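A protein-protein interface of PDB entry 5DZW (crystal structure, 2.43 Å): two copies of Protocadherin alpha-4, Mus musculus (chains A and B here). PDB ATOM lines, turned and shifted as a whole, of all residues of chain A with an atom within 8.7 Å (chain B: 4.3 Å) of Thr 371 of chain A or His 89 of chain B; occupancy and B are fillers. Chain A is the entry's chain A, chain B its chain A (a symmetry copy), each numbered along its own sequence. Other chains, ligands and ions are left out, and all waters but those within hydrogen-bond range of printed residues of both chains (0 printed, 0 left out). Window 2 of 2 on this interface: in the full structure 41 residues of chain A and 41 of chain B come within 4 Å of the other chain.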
ATOM      1  N   LYS A 324      -1.550 -16.645  11.501  1.00  0.00           N
ATOM      2  CA  LYS A 324      -2.959 -16.958  11.712  1.00  0.00           C
ATOM      3  C   LYS A 324      -3.164 -18.180  12.603  1.00  0.00           C
ATOM      4  O   LYS A 324      -4.248 -18.377  13.154  1.00  0.00           O
ATOM      5  CB  LYS A 324      -3.660 -17.174  10.369  1.00  0.00           C
ATOM      6  CG  LYS A 324      -3.844 -15.904   9.559  1.00  0.00           C
ATOM      7  CD  LYS A 324      -4.684 -16.163   8.324  1.00  0.00           C
ATOM      8  CE  LYS A 324      -5.171 -14.867   7.704  1.00  0.00           C
ATOM      9  NZ  LYS A 324      -6.118 -15.120   6.585  1.00  0.00           N
ATOM     10  N   VAL A 339       3.014 -29.114  11.458  1.00  0.00           N
ATOM     11  CA  VAL A 339       2.838 -27.688  11.221  1.00  0.00           C
ATOM     12  C   VAL A 339       2.900 -26.910  12.530  1.00  0.00           C
ATOM     13  O   VAL A 339       2.236 -27.258  13.505  1.00  0.00           O
ATOM     14  CB  VAL A 339       1.504 -27.397  10.515  1.00  0.00           C
ATOM     15  CG1 VAL A 339       1.390 -25.917  10.183  1.00  0.00           C
ATOM     16  CG2 VAL A 339       1.377 -28.240   9.256  1.00  0.00           C
ATOM     17  N   ALA A 341       3.140 -22.994  12.584  1.00  0.00           N
ATOM     18  CA  ALA A 341       2.353 -21.785  12.394  1.00  0.00           C
ATOM     19  C   ALA A 341       1.918 -21.629  10.945  1.00  0.00           C
ATOM     20  O   ALA A 341       2.617 -22.056  10.025  1.00  0.00           O
ATOM     21  CB  ALA A 341       3.144 -20.564  12.841  1.00  0.00           C
ATOM     22  N   LEU A 342       0.753 -21.021  10.750  1.00  0.00           N
ATOM     23  CA  LEU A 342       0.287 -20.670   9.415  1.00  0.00           C
ATOM     24  C   LEU A 342       0.573 -19.199   9.155  1.00  0.00           C
ATOM     25  O   LEU A 342       0.258 -18.343   9.983  1.00  0.00           O
ATOM     26  CB  LEU A 342      -1.206 -20.965   9.259  1.00  0.00           C
ATOM     27  CG  LEU A 342      -1.820 -20.658   7.891  1.00  0.00           C
ATOM     28  CD1 LEU A 342      -1.105 -21.426   6.791  1.00  0.00           C
ATOM     29  CD2 LEU A 342      -3.307 -20.976   7.888  1.00  0.00           C
ATOM     30  N   ILE A 343       1.177 -18.910   8.008  1.00  0.00           N
ATOM     31  CA  ILE A 343       1.566 -17.545   7.676  1.00  0.00           C
ATOM     32  C   ILE A 343       0.746 -16.993   6.516  1.00  0.00           C
ATOM     33  O   ILE A 343       0.552 -17.665   5.503  1.00  0.00           O
ATOM     34  CB  ILE A 343       3.062 -17.461   7.315  1.00  0.00           C
ATOM     35  CG1 ILE A 343       3.897 -18.252   8.323  1.00  0.00           C
ATOM     36  CG2 ILE A 343       3.517 -16.012   7.248  1.00  0.00           C
ATOM     37  CD1 ILE A 343       5.386 -18.188   8.069  1.00  0.00           C
ATOM     38  N   SER A 344       0.265 -15.764   6.674  1.00  0.00           N
ATOM     39  CA  SER A 344      -0.476 -15.086   5.618  1.00  0.00           C
ATOM     40  C   SER A 344       0.240 -13.810   5.197  1.00  0.00           C
ATOM     41  O   SER A 344       0.701 -13.038   6.041  1.00  0.00           O
ATOM     42  CB  SER A 344      -1.900 -14.767   6.074  1.00  0.00           C
ATOM     43  OG  SER A 344      -2.634 -14.125   5.046  1.00  0.00           O
ATOM     44  N   LEU A 368       9.816 -23.726   5.331  1.00  0.00           N
ATOM     45  CA  LEU A 368       8.759 -22.854   4.831  1.00  0.00           C
ATOM     46  C   LEU A 368       8.247 -23.353   3.481  1.00  0.00           C
ATOM     47  O   LEU A 368       9.025 -23.534   2.545  1.00  0.00           O
ATOM     48  CB  LEU A 368       9.272 -21.421   4.708  1.00  0.00           C
ATOM     49  CG  LEU A 368       8.223 -20.331   4.508  1.00  0.00           C
ATOM     50  CD1 LEU A 368       7.241 -20.337   5.664  1.00  0.00           C
ATOM     51  CD2 LEU A 368       8.896 -18.976   4.378  1.00  0.00           C
ATOM     52  N   VAL A 369       6.940 -23.574   3.381  1.00  0.00           N
ATOM     53  CA  VAL A 369       6.365 -24.138   2.164  1.00  0.00           C
ATOM     54  C   VAL A 369       5.106 -23.387   1.722  1.00  0.00           C
ATOM     55  O   VAL A 369       4.287 -22.980   2.549  1.00  0.00           O
ATOM     56  CB  VAL A 369       6.042 -25.641   2.352  1.00  0.00           C
ATOM     57  CG1 VAL A 369       5.043 -25.843   3.483  1.00  0.00           C
ATOM     58  CG2 VAL A 369       5.532 -26.259   1.055  1.00  0.00           C
ATOM     59  N   SER A 370       4.970 -23.193   0.413  1.00  0.00           N
ATOM     60  CA  SER A 370       3.805 -22.522  -0.150  1.00  0.00           C
ATOM     61  C   SER A 370       2.641 -23.491  -0.324  1.00  0.00           C
ATOM     62  O   SER A 370       2.725 -24.442  -1.100  1.00  0.00           O
ATOM     63  CB  SER A 370       4.152 -21.881  -1.496  1.00  0.00           C
ATOM     64  OG  SER A 370       5.241 -20.982  -1.375  1.00  0.00           O
ATOM     65  N   THR A 371       1.556 -23.241   0.400  1.00  0.00           N
ATOM     66  CA  THR A 371       0.357 -24.066   0.297  1.00  0.00           C
ATOM     67  C   THR A 371      -0.624 -23.460  -0.699  1.00  0.00           C
ATOM     68  O   THR A 371      -1.326 -24.175  -1.413  1.00  0.00           O
ATOM     69  CB  THR A 371      -0.340 -24.225   1.661  1.00  0.00           C
ATOM     70  OG1 THR A 371      -0.816 -22.950   2.108  1.00  0.00           O
ATOM     71  CG2 THR A 371       0.625 -24.790   2.689  1.00  0.00           C
ATOM     72  N   PHE A 372      -0.660 -22.131  -0.738  1.00  0.00           N
ATOM     73  CA  PHE A 372      -1.547 -21.395  -1.630  1.00  0.00           C
ATOM     74  C   PHE A 372      -0.971 -20.003  -1.870  1.00  0.00           C
ATOM     75  O   PHE A 372       0.002 -19.615  -1.221  1.00  0.00           O
ATOM     76  CB  PHE A 372      -2.959 -21.310  -1.037  1.00  0.00           C
ATOM     77  CG  PHE A 372      -4.019 -20.912  -2.026  1.00  0.00           C
ATOM     78  CD1 PHE A 372      -4.460 -21.806  -2.989  1.00  0.00           C
ATOM     79  CD2 PHE A 372      -4.588 -19.650  -1.983  1.00  0.00           C
ATOM     80  CE1 PHE A 372      -5.439 -21.445  -3.896  1.00  0.00           C
ATOM     81  CE2 PHE A 372      -5.567 -19.284  -2.888  1.00  0.00           C
ATOM     82  CZ  PHE A 372      -5.993 -20.183  -3.846  1.00  0.00           C
ATOM     83  N   LYS A 373      -1.563 -19.263  -2.803  1.00  0.00           N
ATOM     84  CA  LYS A 373      -1.111 -17.911  -3.122  1.00  0.00           C
ATOM     85  C   LYS A 373      -1.068 -17.020  -1.883  1.00  0.00           C
ATOM     86  O   LYS A 373      -2.081 -16.840  -1.204  1.00  0.00           O
ATOM     87  CB  LYS A 373      -2.015 -17.284  -4.185  1.00  0.00           C
ATOM     88  N   ASN A 374       0.114 -16.478  -1.599  1.00  0.00           N
ATOM     89  CA  ASN A 374       0.347 -15.621  -0.436  1.00  0.00           C
ATOM     90  C   ASN A 374       0.067 -16.323   0.889  1.00  0.00           C
ATOM     91  O   ASN A 374      -0.261 -15.678   1.885  1.00  0.00           O
ATOM     92  CB  ASN A 374      -0.495 -14.344  -0.529  1.00  0.00           C
ATOM     93  CG  ASN A 374      -0.182 -13.526  -1.767  1.00  0.00           C
ATOM     94  OD1 ASN A 374       0.948 -13.524  -2.254  1.00  0.00           O
ATOM     95  ND2 ASN A 374      -1.186 -12.826  -2.282  1.00  0.00           N
ATOM     96  N   TYR A 375       0.200 -17.646   0.900  1.00  0.00           N
ATOM     97  CA  TYR A 375      -0.004 -18.419   2.119  1.00  0.00           C
ATOM     98  C   TYR A 375       1.130 -19.405   2.364  1.00  0.00           C
ATOM     99  O   TYR A 375       1.503 -20.173   1.478  1.00  0.00           O
ATOM    100  CB  TYR A 375      -1.337 -19.165   2.070  1.00  0.00           C
ATOM    101  CG  TYR A 375      -2.467 -18.418   2.731  1.00  0.00           C
ATOM    102  CD1 TYR A 375      -2.579 -18.379   4.116  1.00  0.00           C
ATOM    103  CD2 TYR A 375      -3.424 -17.754   1.976  1.00  0.00           C
ATOM    104  CE1 TYR A 375      -3.611 -17.698   4.728  1.00  0.00           C
ATOM    105  CE2 TYR A 375      -4.460 -17.069   2.581  1.00  0.00           C
ATOM    106  CZ  TYR A 375      -4.548 -17.046   3.957  1.00  0.00           C
ATOM    107  OH  TYR A 375      -5.578 -16.367   4.566  1.00  0.00           O
ATOM    108  N   TYR A 376       1.668 -19.378   3.578  1.00  0.00           N
ATOM    109  CA  TYR A 376       2.768 -20.257   3.949  1.00  0.00           C
ATOM    110  C   TYR A 376       2.501 -20.953   5.279  1.00  0.00           C
ATOM    111  O   TYR A 376       1.881 -20.381   6.175  1.00  0.00           O
ATOM    112  CB  TYR A 376       4.077 -19.468   4.035  1.00  0.00           C
ATOM    113  CG  TYR A 376       4.491 -18.804   2.743  1.00  0.00           C
ATOM    114  CD1 TYR A 376       5.406 -19.408   1.893  1.00  0.00           C
ATOM    115  CD2 TYR A 376       3.974 -17.567   2.377  1.00  0.00           C
ATOM    116  CE1 TYR A 376       5.794 -18.802   0.712  1.00  0.00           C
ATOM    117  CE2 TYR A 376       4.353 -16.954   1.198  1.00  0.00           C
ATOM    118  CZ  TYR A 376       5.262 -17.575   0.368  1.00  0.00           C
ATOM    119  OH  TYR A 376       5.642 -16.966  -0.805  1.00  0.00           O
ATOM    120  N   SER A 377       2.967 -22.190   5.403  1.00  0.00           N
ATOM    121  CA  SER A 377       2.906 -22.895   6.676  1.00  0.00           C
ATOM    122  C   SER A 377       4.316 -23.235   7.135  1.00  0.00           C
ATOM    123  O   SER A 377       5.130 -23.721   6.351  1.00  0.00           O
ATOM    124  CB  SER A 377       2.051 -24.161   6.567  1.00  0.00           C
ATOM    125  OG  SER A 377       2.609 -25.080   5.648  1.00  0.00           O
ATOM    126  N   LEU A 378       4.606 -22.961   8.403  1.00  0.00           N
ATOM    127  CA  LEU A 378       5.926 -23.238   8.954  1.00  0.00           C
ATOM    128  C   LEU A 378       6.018 -24.692   9.401  1.00  0.00           C
ATOM    129  O   LEU A 378       5.602 -25.043  10.505  1.00  0.00           O
ATOM    130  CB  LEU A 378       6.232 -22.298  10.121  1.00  0.00           C
ATOM    131  CG  LEU A 378       7.659 -22.353  10.671  1.00  0.00           C
ATOM    132  CD1 LEU A 378       8.668 -22.116   9.560  1.00  0.00           C
ATOM    133  CD2 LEU A 378       7.841 -21.338  11.787  1.00  0.00           C
ATOM    134  N   VAL A 379       6.568 -25.533   8.531  1.00  0.00           N
ATOM    135  CA  VAL A 379       6.608 -26.970   8.765  1.00  0.00           C
ATOM    136  C   VAL A 379       7.938 -27.420   9.364  1.00  0.00           C
ATOM    137  O   VAL A 379       9.005 -27.009   8.911  1.00  0.00           O
ATOM    138  CB  VAL A 379       6.355 -27.744   7.456  1.00  0.00           C
ATOM    139  CG1 VAL A 379       6.368 -29.240   7.704  1.00  0.00           C
ATOM    140  CG2 VAL A 379       5.033 -27.319   6.842  1.00  0.00           C
ATOM    141  N   GLN B   1      -5.912 -26.478  -2.842  1.00  0.00           N
ATOM    142  CA  GLN B   1      -6.896 -25.598  -3.461  1.00  0.00           C
ATOM    143  C   GLN B   1      -8.141 -26.362  -3.907  1.00  0.00           C
ATOM    144  O   GLN B   1      -8.101 -27.139  -4.860  1.00  0.00           O
ATOM    145  CB  GLN B   1      -6.272 -24.850  -4.648  1.00  0.00           C
ATOM    146  CG  GLN B   1      -5.301 -25.669  -5.495  1.00  0.00           C
ATOM    147  CD  GLN B   1      -5.961 -26.333  -6.691  1.00  0.00           C
ATOM    148  OE1 GLN B   1      -5.804 -27.535  -6.915  1.00  0.00           O
ATOM    149  NE2 GLN B   1      -6.700 -25.551  -7.470  1.00  0.00           N
ATOM    150  N   ILE B   2      -9.247 -26.144  -3.200  1.00  0.00           N
ATOM    151  CA  ILE B   2     -10.535 -26.680  -3.636  1.00  0.00           C
ATOM    152  C   ILE B   2     -11.507 -25.526  -3.888  1.00  0.00           C
ATOM    153  O   ILE B   2     -11.686 -24.652  -3.038  1.00  0.00           O
ATOM    154  CB  ILE B   2     -11.120 -27.676  -2.606  1.00  0.00           C
ATOM    155  CG1 ILE B   2     -12.601 -27.948  -2.886  1.00  0.00           C
ATOM    156  CG2 ILE B   2     -10.924 -27.171  -1.193  1.00  0.00           C
ATOM    157  CD1 ILE B   2     -12.849 -28.718  -4.165  1.00  0.00           C
ATOM    158  N   HIS B  76     -12.010 -16.539   0.597  1.00  0.00           N
ATOM    159  CA  HIS B  76     -10.958 -17.509   0.858  1.00  0.00           C
ATOM    160  C   HIS B  76     -11.087 -18.088   2.260  1.00  0.00           C
ATOM    161  O   HIS B  76     -10.876 -17.394   3.256  1.00  0.00           O
ATOM    162  CB  HIS B  76      -9.578 -16.877   0.678  1.00  0.00           C
ATOM    163  CG  HIS B  76      -8.450 -17.847   0.835  1.00  0.00           C
ATOM    164  ND1 HIS B  76      -8.092 -18.737  -0.154  1.00  0.00           N
ATOM    165  CD2 HIS B  76      -7.610 -18.079   1.872  1.00  0.00           C
ATOM    166  CE1 HIS B  76      -7.074 -19.470   0.263  1.00  0.00           C
ATOM    167  NE2 HIS B  76      -6.763 -19.091   1.488  1.00  0.00           N
ATOM    168  N   LEU B  77     -11.440 -19.367   2.329  1.00  0.00           N
ATOM    169  CA  LEU B  77     -11.553 -20.063   3.602  1.00  0.00           C
ATOM    170  C   LEU B  77     -10.354 -20.962   3.856  1.00  0.00           C
ATOM    171  O   LEU B  77     -10.020 -21.835   3.045  1.00  0.00           O
ATOM    172  CB  LEU B  77     -12.835 -20.894   3.659  1.00  0.00           C
ATOM    173  CG  LEU B  77     -14.173 -20.166   3.755  1.00  0.00           C
ATOM    174  CD1 LEU B  77     -15.296 -21.182   3.831  1.00  0.00           C
ATOM    175  CD2 LEU B  77     -14.204 -19.238   4.958  1.00  0.00           C
ATOM    176  N   PHE B  88      -5.918 -26.747   5.221  1.00  0.00           N
ATOM    177  CA  PHE B  88      -6.399 -26.862   3.850  1.00  0.00           C
ATOM    178  C   PHE B  88      -6.894 -25.511   3.334  1.00  0.00           C
ATOM    179  O   PHE B  88      -7.156 -24.598   4.121  1.00  0.00           O
ATOM    180  CB  PHE B  88      -7.517 -27.904   3.764  1.00  0.00           C
ATOM    181  CG  PHE B  88      -7.178 -29.218   4.413  1.00  0.00           C
ATOM    182  CD1 PHE B  88      -6.531 -30.213   3.699  1.00  0.00           C
ATOM    183  CD2 PHE B  88      -7.514 -29.460   5.735  1.00  0.00           C
ATOM    184  CE1 PHE B  88      -6.221 -31.422   4.293  1.00  0.00           C
ATOM    185  CE2 PHE B  88      -7.208 -30.668   6.334  1.00  0.00           C
ATOM    186  CZ  PHE B  88      -6.561 -31.650   5.613  1.00  0.00           C
ATOM    187  N   HIS B  89      -7.025 -25.388   2.015  1.00  0.00           N
ATOM    188  CA  HIS B  89      -7.471 -24.135   1.409  1.00  0.00           C
ATOM    189  C   HIS B  89      -8.643 -24.318   0.444  1.00  0.00           C
ATOM    190  O   HIS B  89      -8.545 -25.042  -0.556  1.00  0.00           O
ATOM    191  CB  HIS B  89      -6.310 -23.453   0.683  1.00  0.00           C
ATOM    192  CG  HIS B  89      -5.234 -22.957   1.599  1.00  0.00           C
ATOM    193  ND1 HIS B  89      -5.436 -21.931   2.496  1.00  0.00           N
ATOM    194  CD2 HIS B  89      -3.946 -23.343   1.753  1.00  0.00           C
ATOM    195  CE1 HIS B  89      -4.320 -21.708   3.166  1.00  0.00           C
ATOM    196  NE2 HIS B  89      -3.399 -22.551   2.734  1.00  0.00           N
ATOM    197  N   VAL B  90      -9.749 -23.644   0.749  1.00  0.00           N
ATOM    198  CA  VAL B  90     -10.920 -23.669  -0.118  1.00  0.00           C
ATOM    199  C   VAL B  90     -11.320 -22.260  -0.532  1.00  0.00           C
ATOM    200  O   VAL B  90     -11.581 -21.406   0.309  1.00  0.00           O
ATOM    201  CB  VAL B  90     -12.120 -24.367   0.561  1.00  0.00           C
ATOM    202  CG1 VAL B  90     -12.214 -23.974   2.024  1.00  0.00           C
ATOM    203  CG2 VAL B  90     -13.416 -24.041  -0.172  1.00  0.00           C
ATOM    204  N   GLU B  91     -11.355 -22.018  -1.836  1.00  0.00           N
ATOM    205  CA  GLU B  91     -11.754 -20.714  -2.349  1.00  0.00           C
ATOM    206  C   GLU B  91     -13.118 -20.809  -3.017  1.00  0.00           C
ATOM    207  O   GLU B  91     -13.318 -21.621  -3.919  1.00  0.00           O
ATOM    208  CB  GLU B  91     -10.713 -20.180  -3.333  1.00  0.00           C
ATOM    209  CG  GLU B  91     -11.020 -18.797  -3.876  1.00  0.00           C
ATOM    210  CD  GLU B  91      -9.995 -18.336  -4.892  1.00  0.00           C
ATOM    211  OE1 GLU B  91      -9.061 -19.112  -5.184  1.00  0.00           O
ATOM    212  OE2 GLU B  91     -10.121 -17.201  -5.399  1.00  0.00           O
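OG1 of Thr 371 of chain A lies within hydrogen-bond range of NE2 of His 89 of chain B (2.7 Å).
OH of Tyr 375 of chain A is in hydrogen-bond range of NZ of Lys 324 of chain A (2.4 Å).
O of His 89 of chain B is in hydrogen-bond range of N of Ile 2 of chain B (2.9 Å).
The backbone NH (N) of Glu 91 of chain B sits at hydrogen-bond distance from the backbone carbonyl oxygen (O) of Ile 2 of chain B.
NE2 of His 76 of chain B sits at hydrogen-bond distance from ND1 of His 89 of chain B (3.3 Å).
Among the printed residues, merely in contact across the chains: Phe 372 of chain A with Gln 1 of chain B, Phe 372 of chain A with His 76 of chain B, Phe 372 of chain A with His 89 of chain B, Phe 372 of chain A with Glu 91 of chain B, Tyr 375 of chain A with His 76 of chain B and Tyr 375 of chain A with His 89 of chain B.
Leu 368 of chain A touches none of the printed residues of chain B.
Thr 371 of chain A touches just one residue of chain B: His 89 (2.7 Å).
Of the printed residues of chain B, Phe 372 of chain A touches Gln 1 (3.6 Å), His 76 (3.4 Å), His 89 (3.6 Å) and Glu 91 (3.5 Å).
Of the printed residues of chain B, Tyr 375 of chain A touches His 76 (3.3 Å) and His 89 (3.8 Å).
Leu 378 of chain A touches none of the printed residues of chain B.
Printed residues of chain A within 4 Å of Gln 1 of chain B: Phe 372.
Of the printed residues of chain A, His 76 of chain B touches Phe 372 (3.4 Å) and Tyr 375 (3.3 Å).
Printed residues of chain A within 4 Å of Glu 91 of chain B: Phe 372 (3.5 Å).
The nearest printed residue of chain B that does not touch Thr 371 of chain A is Gln 1 of chain B (5.3 Å).
The nearest printed residue of chain A that does not touch His 76 of chain B is Lys 324 of chain A (5.8 Å).
Of the 18 printed residues of chain A, 3 touch a printed residue of chain B.
Printed residues of chain B that touch a printed residue of chain A: Gln 1, His 76, His 89 and Glu 91.
Hydrophobic or aromatic side chains of chain B within 4 Å of the printed part of chain A: His 76 and His 89.
No position is printed for both chains.
Of the 7 pairs that touch across the chains among the printed residues, none has its exchanged pair printed and touching as well.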
